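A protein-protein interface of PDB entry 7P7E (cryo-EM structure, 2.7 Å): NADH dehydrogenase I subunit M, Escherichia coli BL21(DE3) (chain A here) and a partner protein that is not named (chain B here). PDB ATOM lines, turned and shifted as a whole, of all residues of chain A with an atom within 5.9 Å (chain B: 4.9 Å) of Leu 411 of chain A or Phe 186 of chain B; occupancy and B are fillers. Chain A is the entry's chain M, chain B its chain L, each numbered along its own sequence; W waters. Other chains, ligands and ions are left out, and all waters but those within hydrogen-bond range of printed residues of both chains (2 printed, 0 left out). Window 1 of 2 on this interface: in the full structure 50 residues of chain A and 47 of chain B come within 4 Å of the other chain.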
ATOM      1  N   PHE A 325     -18.337  22.134 -15.291  1.00  0.00           N
ATOM      2  CA  PHE A 325     -17.505  20.990 -15.688  1.00  0.00           C
ATOM      3  C   PHE A 325     -18.168  19.659 -15.329  1.00  0.00           C
ATOM      4  O   PHE A 325     -18.228  18.730 -16.151  1.00  0.00           O
ATOM      5  CB  PHE A 325     -16.137  21.067 -15.014  1.00  0.00           C
ATOM      6  CG  PHE A 325     -15.125  21.874 -15.760  1.00  0.00           C
ATOM      7  CD1 PHE A 325     -14.516  21.369 -16.893  1.00  0.00           C
ATOM      8  CD2 PHE A 325     -14.755  23.128 -15.305  1.00  0.00           C
ATOM      9  CE1 PHE A 325     -13.572  22.108 -17.568  1.00  0.00           C
ATOM     10  CE2 PHE A 325     -13.814  23.873 -15.980  1.00  0.00           C
ATOM     11  CZ  PHE A 325     -13.223  23.363 -17.113  1.00  0.00           C
ATOM     12  N   GLY A 406      -9.726  15.234 -11.129  1.00  0.00           N
ATOM     13  CA  GLY A 406     -11.126  15.231 -11.524  1.00  0.00           C
ATOM     14  C   GLY A 406     -11.367  15.936 -12.844  1.00  0.00           C
ATOM     15  O   GLY A 406     -12.001  15.382 -13.745  1.00  0.00           O
ATOM     16  N   GLU A 407     -10.806  17.139 -13.000  1.00  0.00           N
ATOM     17  CA  GLU A 407     -11.056  17.951 -14.185  1.00  0.00           C
ATOM     18  C   GLU A 407     -10.497  17.293 -15.437  1.00  0.00           C
ATOM     19  O   GLU A 407     -11.188  17.178 -16.452  1.00  0.00           O
ATOM     20  CB  GLU A 407     -10.439  19.338 -13.997  1.00  0.00           C
ATOM     21  CG  GLU A 407     -11.264  20.468 -14.573  1.00  0.00           C
ATOM     22  CD  GLU A 407     -12.316  20.960 -13.598  1.00  0.00           C
ATOM     23  OE1 GLU A 407     -12.070  21.975 -12.913  1.00  0.00           O
ATOM     24  OE2 GLU A 407     -13.380  20.316 -13.495  1.00  0.00           O
ATOM     25  N   PHE A 408      -9.250  16.824 -15.377  1.00  0.00           N
ATOM     26  CA  PHE A 408      -8.633  16.253 -16.562  1.00  0.00           C
ATOM     27  C   PHE A 408      -9.171  14.868 -16.873  1.00  0.00           C
ATOM     28  O   PHE A 408      -9.196  14.480 -18.038  1.00  0.00           O
ATOM     29  CB  PHE A 408      -7.118  16.213 -16.410  1.00  0.00           C
ATOM     30  CG  PHE A 408      -6.418  17.319 -17.134  1.00  0.00           C
ATOM     31  CD1 PHE A 408      -6.712  18.642 -16.845  1.00  0.00           C
ATOM     32  CD2 PHE A 408      -5.464  17.043 -18.099  1.00  0.00           C
ATOM     33  CE1 PHE A 408      -6.069  19.668 -17.502  1.00  0.00           C
ATOM     34  CE2 PHE A 408      -4.817  18.066 -18.759  1.00  0.00           C
ATOM     35  CZ  PHE A 408      -5.123  19.379 -18.460  1.00  0.00           C
ATOM     36  N   MET A 409      -9.624  14.112 -15.871  1.00  0.00           N
ATOM     37  CA  MET A 409     -10.239  12.828 -16.177  1.00  0.00           C
ATOM     38  C   MET A 409     -11.608  13.032 -16.817  1.00  0.00           C
ATOM     39  O   MET A 409     -11.986  12.300 -17.748  1.00  0.00           O
ATOM     40  CB  MET A 409     -10.310  11.999 -14.899  1.00  0.00           C
ATOM     41  CG  MET A 409      -9.557  10.690 -14.994  1.00  0.00           C
ATOM     42  SD  MET A 409      -9.413   9.835 -13.419  1.00  0.00           S
ATOM     43  CE  MET A 409     -11.104   9.369 -13.149  1.00  0.00           C
ATOM     44  N   ILE A 410     -12.334  14.063 -16.360  1.00  0.00           N
ATOM     45  CA  ILE A 410     -13.553  14.509 -17.032  1.00  0.00           C
ATOM     46  C   ILE A 410     -13.257  14.871 -18.479  1.00  0.00           C
ATOM     47  O   ILE A 410     -13.979  14.469 -19.397  1.00  0.00           O
ATOM     48  CB  ILE A 410     -14.170  15.702 -16.277  1.00  0.00           C
ATOM     49  CG1 ILE A 410     -14.900  15.237 -15.025  1.00  0.00           C
ATOM     50  CG2 ILE A 410     -15.104  16.513 -17.170  1.00  0.00           C
ATOM     51  CD1 ILE A 410     -15.341  16.371 -14.140  1.00  0.00           C
ATOM     52  N   LEU A 411     -12.182  15.626 -18.704  1.00  0.00           N
ATOM     53  CA  LEU A 411     -11.865  16.076 -20.054  1.00  0.00           C
ATOM     54  C   LEU A 411     -11.379  14.936 -20.942  1.00  0.00           C
ATOM     55  O   LEU A 411     -11.660  14.939 -22.139  1.00  0.00           O
ATOM     56  CB  LEU A 411     -10.835  17.202 -20.006  1.00  0.00           C
ATOM     57  CG  LEU A 411     -11.300  18.525 -19.394  1.00  0.00           C
ATOM     58  CD1 LEU A 411     -10.174  19.538 -19.387  1.00  0.00           C
ATOM     59  CD2 LEU A 411     -12.523  19.078 -20.103  1.00  0.00           C
ATOM     60  N   PHE A 412     -10.675  13.949 -20.382  1.00  0.00           N
ATOM     61  CA  PHE A 412     -10.283  12.772 -21.155  1.00  0.00           C
ATOM     62  C   PHE A 412     -11.509  11.990 -21.621  1.00  0.00           C
ATOM     63  O   PHE A 412     -11.646  11.675 -22.812  1.00  0.00           O
ATOM     64  CB  PHE A 412      -9.367  11.876 -20.317  1.00  0.00           C
ATOM     65  CG  PHE A 412      -7.898  12.161 -20.489  1.00  0.00           C
ATOM     66  CD1 PHE A 412      -7.268  11.932 -21.699  1.00  0.00           C
ATOM     67  CD2 PHE A 412      -7.141  12.632 -19.429  1.00  0.00           C
ATOM     68  CE1 PHE A 412      -5.918  12.187 -21.852  1.00  0.00           C
ATOM     69  CE2 PHE A 412      -5.793  12.891 -19.575  1.00  0.00           C
ATOM     70  CZ  PHE A 412      -5.181  12.666 -20.788  1.00  0.00           C
ATOM     71  N   GLY A 413     -12.429  11.696 -20.693  1.00  0.00           N
ATOM     72  CA  GLY A 413     -13.649  10.995 -21.075  1.00  0.00           C
ATOM     73  C   GLY A 413     -14.513  11.793 -22.034  1.00  0.00           C
ATOM     74  O   GLY A 413     -15.069  11.247 -22.995  1.00  0.00           O
ATOM     75  N   SER A 414     -14.616  13.102 -21.803  1.00  0.00           N
ATOM     76  CA  SER A 414     -15.416  13.958 -22.666  1.00  0.00           C
ATOM     77  C   SER A 414     -14.813  14.061 -24.058  1.00  0.00           C
ATOM     78  O   SER A 414     -15.545  14.050 -25.046  1.00  0.00           O
ATOM     79  CB  SER A 414     -15.563  15.340 -22.037  1.00  0.00           C
ATOM     80  OG  SER A 414     -16.184  15.253 -20.770  1.00  0.00           O
ATOM     81  N   PHE A 415     -13.484  14.147 -24.161  1.00  0.00           N
ATOM     82  CA  PHE A 415     -12.847  14.161 -25.471  1.00  0.00           C
ATOM     83  C   PHE A 415     -13.037  12.836 -26.189  1.00  0.00           C
ATOM     84  O   PHE A 415     -13.099  12.807 -27.423  1.00  0.00           O
ATOM     85  CB  PHE A 415     -11.360  14.486 -25.342  1.00  0.00           C
ATOM     86  CG  PHE A 415     -10.728  14.933 -26.629  1.00  0.00           C
ATOM     87  CD1 PHE A 415     -10.753  16.266 -27.000  1.00  0.00           C
ATOM     88  CD2 PHE A 415     -10.118  14.019 -27.473  1.00  0.00           C
ATOM     89  CE1 PHE A 415     -10.181  16.680 -28.184  1.00  0.00           C
ATOM     90  CE2 PHE A 415      -9.546  14.428 -28.658  1.00  0.00           C
ATOM     91  CZ  PHE A 415      -9.577  15.760 -29.013  1.00  0.00           C
ATOM     92  N   GLN A 416     -13.126  11.735 -25.440  1.00  0.00           N
ATOM     93  CA  GLN A 416     -13.557  10.488 -26.061  1.00  0.00           C
ATOM     94  C   GLN A 416     -14.998  10.574 -26.553  1.00  0.00           C
ATOM     95  O   GLN A 416     -15.355   9.912 -27.532  1.00  0.00           O
ATOM     96  CB  GLN A 416     -13.400   9.323 -25.088  1.00  0.00           C
ATOM     97  CG  GLN A 416     -11.966   9.010 -24.725  1.00  0.00           C
ATOM     98  CD  GLN A 416     -11.781   7.567 -24.325  1.00  0.00           C
ATOM     99  OE1 GLN A 416     -11.604   6.695 -25.173  1.00  0.00           O
ATOM    100  NE2 GLN A 416     -11.826   7.303 -23.026  1.00  0.00           N
ATOM    101  N   ILE A 421     -16.692  20.437 -27.085  1.00  0.00           N
ATOM    102  CA  ILE A 421     -17.033  20.873 -25.734  1.00  0.00           C
ATOM    103  C   ILE A 421     -15.820  20.755 -24.818  1.00  0.00           C
ATOM    104  O   ILE A 421     -15.567  21.629 -23.978  1.00  0.00           O
ATOM    105  CB  ILE A 421     -18.240  20.061 -25.222  1.00  0.00           C
ATOM    106  CG1 ILE A 421     -19.526  20.551 -25.889  1.00  0.00           C
ATOM    107  CG2 ILE A 421     -18.381  20.136 -23.712  1.00  0.00           C
ATOM    108  CD1 ILE A 421     -20.386  19.443 -26.448  1.00  0.00           C
ATOM    109  N   THR A 422     -15.022  19.700 -25.008  1.00  0.00           N
ATOM    110  CA  THR A 422     -13.791  19.526 -24.241  1.00  0.00           C
ATOM    111  C   THR A 422     -12.781  20.636 -24.526  1.00  0.00           C
ATOM    112  O   THR A 422     -12.118  21.134 -23.604  1.00  0.00           O
ATOM    113  CB  THR A 422     -13.185  18.160 -24.555  1.00  0.00           C
ATOM    114  OG1 THR A 422     -14.213  17.162 -24.524  1.00  0.00           O
ATOM    115  CG2 THR A 422     -12.107  17.814 -23.556  1.00  0.00           C
ATOM    116  N   SER A 425     -13.949  23.778 -22.873  1.00  0.00           N
ATOM    117  CA  SER A 425     -13.793  23.659 -21.425  1.00  0.00           C
ATOM    118  C   SER A 425     -12.339  23.811 -20.974  1.00  0.00           C
ATOM    119  O   SER A 425     -12.075  24.356 -19.893  1.00  0.00           O
ATOM    120  CB  SER A 425     -14.366  22.322 -20.969  1.00  0.00           C
ATOM    121  OG  SER A 425     -15.597  22.058 -21.616  1.00  0.00           O
ATOM    122  N   THR A 426     -11.379  23.339 -21.771  1.00  0.00           N
ATOM    123  CA  THR A 426      -9.975  23.554 -21.412  1.00  0.00           C
ATOM    124  C   THR A 426      -9.603  25.036 -21.491  1.00  0.00           C
ATOM    125  O   THR A 426      -8.833  25.552 -20.658  1.00  0.00           O
ATOM    126  CB  THR A 426      -9.077  22.708 -22.309  1.00  0.00           C
ATOM    127  OG1 THR A 426      -9.814  21.573 -22.780  1.00  0.00           O
ATOM    128  CG2 THR A 426      -7.867  22.220 -21.538  1.00  0.00           C
ATOM    129  N   LEU A 429     -10.458  26.338 -18.379  1.00  0.00           N
ATOM    130  CA  LEU A 429      -9.398  26.178 -17.378  1.00  0.00           C
ATOM    131  C   LEU A 429      -8.405  27.342 -17.421  1.00  0.00           C
ATOM    132  O   LEU A 429      -7.893  27.778 -16.375  1.00  0.00           O
ATOM    133  CB  LEU A 429      -8.663  24.853 -17.569  1.00  0.00           C
ATOM    134  CG  LEU A 429      -9.281  23.575 -17.008  1.00  0.00           C
ATOM    135  CD1 LEU A 429      -8.558  22.376 -17.581  1.00  0.00           C
ATOM    136  CD2 LEU A 429      -9.215  23.566 -15.491  1.00  0.00           C
ATOM    137  N   ALA B 182      -2.478  19.992 -23.366  1.00  0.00           N
ATOM    138  CA  ALA B 182      -3.561  19.136 -22.893  1.00  0.00           C
ATOM    139  C   ALA B 182      -4.379  18.588 -24.053  1.00  0.00           C
ATOM    140  O   ALA B 182      -4.822  17.433 -24.013  1.00  0.00           O
ATOM    141  CB  ALA B 182      -4.454  19.912 -21.927  1.00  0.00           C
ATOM    142  N   PHE B 183      -4.602  19.408 -25.085  1.00  0.00           N
ATOM    143  CA  PHE B 183      -5.249  18.917 -26.302  1.00  0.00           C
ATOM    144  C   PHE B 183      -4.454  17.779 -26.925  1.00  0.00           C
ATOM    145  O   PHE B 183      -5.030  16.772 -27.363  1.00  0.00           O
ATOM    146  CB  PHE B 183      -5.403  20.038 -27.326  1.00  0.00           C
ATOM    147  CG  PHE B 183      -6.335  21.122 -26.910  1.00  0.00           C
ATOM    148  CD1 PHE B 183      -7.366  20.866 -26.030  1.00  0.00           C
ATOM    149  CD2 PHE B 183      -6.182  22.403 -27.411  1.00  0.00           C
ATOM    150  CE1 PHE B 183      -8.219  21.865 -25.652  1.00  0.00           C
ATOM    151  CE2 PHE B 183      -7.038  23.408 -27.034  1.00  0.00           C
ATOM    152  CZ  PHE B 183      -8.057  23.139 -26.154  1.00  0.00           C
ATOM    153  N   ALA B 184      -3.125  17.930 -26.973  1.00  0.00           N
ATOM    154  CA  ALA B 184      -2.271  16.862 -27.496  1.00  0.00           C
ATOM    155  C   ALA B 184      -2.417  15.582 -26.680  1.00  0.00           C
ATOM    156  O   ALA B 184      -2.497  14.482 -27.244  1.00  0.00           O
ATOM    157  CB  ALA B 184      -0.811  17.307 -27.512  1.00  0.00           C
ATOM    158  N   LEU B 185      -2.458  15.713 -25.350  1.00  0.00           N
ATOM    159  CA  LEU B 185      -2.619  14.547 -24.480  1.00  0.00           C
ATOM    160  C   LEU B 185      -3.961  13.855 -24.704  1.00  0.00           C
ATOM    161  O   LEU B 185      -4.029  12.618 -24.749  1.00  0.00           O
ATOM    162  CB  LEU B 185      -2.479  14.962 -23.017  1.00  0.00           C
ATOM    163  CG  LEU B 185      -1.123  14.743 -22.352  1.00  0.00           C
ATOM    164  CD1 LEU B 185      -0.093  15.724 -22.878  1.00  0.00           C
ATOM    165  CD2 LEU B 185      -1.249  14.863 -20.852  1.00  0.00           C
ATOM    166  N   PHE B 186      -5.039  14.638 -24.836  1.00  0.00           N
ATOM    167  CA  PHE B 186      -6.361  14.056 -25.067  1.00  0.00           C
ATOM    168  C   PHE B 186      -6.406  13.312 -26.393  1.00  0.00           C
ATOM    169  O   PHE B 186      -6.948  12.203 -26.469  1.00  0.00           O
ATOM    170  CB  PHE B 186      -7.451  15.132 -25.050  1.00  0.00           C
ATOM    171  CG  PHE B 186      -7.516  15.930 -23.781  1.00  0.00           C
ATOM    172  CD1 PHE B 186      -7.144  15.378 -22.567  1.00  0.00           C
ATOM    173  CD2 PHE B 186      -7.964  17.240 -23.805  1.00  0.00           C
ATOM    174  CE1 PHE B 186      -7.202  16.120 -21.410  1.00  0.00           C
ATOM    175  CE2 PHE B 186      -8.024  17.985 -22.649  1.00  0.00           C
ATOM    176  CZ  PHE B 186      -7.639  17.424 -21.451  1.00  0.00           C
ATOM    177  N   ILE B 187      -5.822  13.905 -27.442  1.00  0.00           N
ATOM    178  CA  ILE B 187      -5.789  13.260 -28.754  1.00  0.00           C
ATOM    179  C   ILE B 187      -5.009  11.953 -28.687  1.00  0.00           C
ATOM    180  O   ILE B 187      -5.452  10.915 -29.199  1.00  0.00           O
ATOM    181  CB  ILE B 187      -5.189  14.211 -29.806  1.00  0.00           C
ATOM    182  CG1 ILE B 187      -6.113  15.396 -30.071  1.00  0.00           C
ATOM    183  CG2 ILE B 187      -4.923  13.476 -31.104  1.00  0.00           C
ATOM    184  CD1 ILE B 187      -5.414  16.564 -30.730  1.00  0.00           C
ATOM    185  N   LEU B 188      -3.844  11.980 -28.034  1.00  0.00           N
ATOM    186  CA  LEU B 188      -2.984  10.803 -28.023  1.00  0.00           C
ATOM    187  C   LEU B 188      -3.588   9.671 -27.203  1.00  0.00           C
ATOM    188  O   LEU B 188      -3.451   8.499 -27.574  1.00  0.00           O
ATOM    189  CB  LEU B 188      -1.594  11.173 -27.513  1.00  0.00           C
ATOM    190  CG  LEU B 188      -0.723  11.815 -28.596  1.00  0.00           C
ATOM    191  CD1 LEU B 188       0.483  12.506 -28.004  1.00  0.00           C
ATOM    192  CD2 LEU B 188      -0.299  10.782 -29.623  1.00  0.00           C
ATOM    193  N   TYR B 189      -4.276   9.985 -26.100  1.00  0.00           N
ATOM    194  CA  TYR B 189      -4.954   8.915 -25.374  1.00  0.00           C
ATOM    195  C   TYR B 189      -6.153   8.384 -26.152  1.00  0.00           C
ATOM    196  O   TYR B 189      -6.388   7.170 -26.177  1.00  0.00           O
ATOM    197  CB  TYR B 189      -5.406   9.361 -23.987  1.00  0.00           C
ATOM    198  CG  TYR B 189      -6.278   8.305 -23.340  1.00  0.00           C
ATOM    199  CD1 TYR B 189      -5.740   7.085 -22.950  1.00  0.00           C
ATOM    200  CD2 TYR B 189      -7.644   8.502 -23.169  1.00  0.00           C
ATOM    201  CE1 TYR B 189      -6.528   6.105 -22.384  1.00  0.00           C
ATOM    202  CE2 TYR B 189      -8.440   7.526 -22.607  1.00  0.00           C
ATOM    203  CZ  TYR B 189      -7.876   6.329 -22.217  1.00  0.00           C
ATOM    204  OH  TYR B 189      -8.661   5.355 -21.650  1.00  0.00           O
ATOM    205  N   ASN B 190      -6.931   9.273 -26.781  1.00  0.00           N
ATOM    206  CA  ASN B 190      -8.107   8.827 -27.522  1.00  0.00           C
ATOM    207  C   ASN B 190      -7.728   7.962 -28.715  1.00  0.00           C
ATOM    208  O   ASN B 190      -8.495   7.074 -29.107  1.00  0.00           O
ATOM    209  CB  ASN B 190      -8.920  10.034 -27.985  1.00  0.00           C
ATOM    210  CG  ASN B 190     -10.255   9.643 -28.583  1.00  0.00           C
ATOM    211  OD1 ASN B 190     -10.831   8.617 -28.229  1.00  0.00           O
ATOM    212  ND2 ASN B 190     -10.750  10.460 -29.502  1.00  0.00           N
HETATM  213  O   HOH W   1      -9.272  11.395 -24.466  1.00  0.00           O
HETATM  214  O   HOH W   2     -11.260   4.954 -21.535  1.00  0.00           O
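Leu 411 of chain A touches just one residue of chain B: Phe 186.
Printed residues of chain A within 4 Å of Phe 186 of chain B: Phe 408 (3.9 Å), Leu 411 (3.5 Å), Phe 412 (3.5 Å) and Phe 415 (3.6 Å).
Of the printed residues of chain A, Leu 185 of chain B touches Phe 412 (3.5 Å).
Of the printed residues of chain B, Phe 412 of chain A touches Leu 185, Phe 186 and Tyr 189.
Of the printed residues of chain A, Ala 182 of chain B touches Phe 408 (3.6 Å).
The nearest printed residue of chain B that does not touch Leu 411 of chain A is Ala 182 of chain B (6.3 Å).
The backbone NH of Phe 415 of chain A sits at hydrogen-bond distance from the side-chain hydroxyl of Thr 422 of chain A (3.1 Å).
O of Thr 422 of chain A sits at hydrogen-bond distance from OG1 of Thr 426 of chain A, 2.5 Å away.
Phe 408 of chain A touches Ala 182 of chain B (CZ to CB, 3.6 Å).
Phe 408 of chain A touches Phe 186 of chain B.
Leu 411 of chain A touches Phe 186 of chain B.
CE1 of Phe 412 of chain A touches CD1 of Phe 186 of chain B (3.5 Å).
Tyr 189 of chain B touches Phe 412 of chain A (CB to CE1, 3.6 Å).
Phe 186 of chain B touches Phe 415 of chain A (CB to CG, 3.6 Å).
O of Phe 415 of chain A touches ND2 of Asn 190 of chain B, at 3.9 Å.
Gln 416 of chain A touches Tyr 189 of chain B (NE2 to CE2, 3.4 Å).
Gln 416 of chain A touches Asn 190 of chain B (OE1 to OD1, 3.7 Å).
OG1 of Thr 426 of chain A touches CE1 of Phe 183 of chain B, 3.3 Å away.
Water W2 bridges the side-chain hydroxyl of Tyr 189 of chain B and the side-chain amide nitrogen of Gln 416 of chain A.
Water W1 lies within hydrogen-bond range of O of Phe 412 of chain A (2.9 Å) and O of Phe 186 of chain B (3.2 Å).
Of the 17 printed residues of chain A, 6 touch a printed residue of chain B.
Hydrophobic or aromatic side chains of chain A that line the printed part of chain B: Phe 408, Leu 411, Phe 412 and Phe 415.
Of the 9 printed residues of chain B, 7 touch a printed residue of chain A.
Among the printed residues, 12 pairs touch across the chains.
Among the printed residues, no Asp or Glu carboxylate lies within 4 Å of a Lys or Arg side-chain nitrogen of the other chain.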
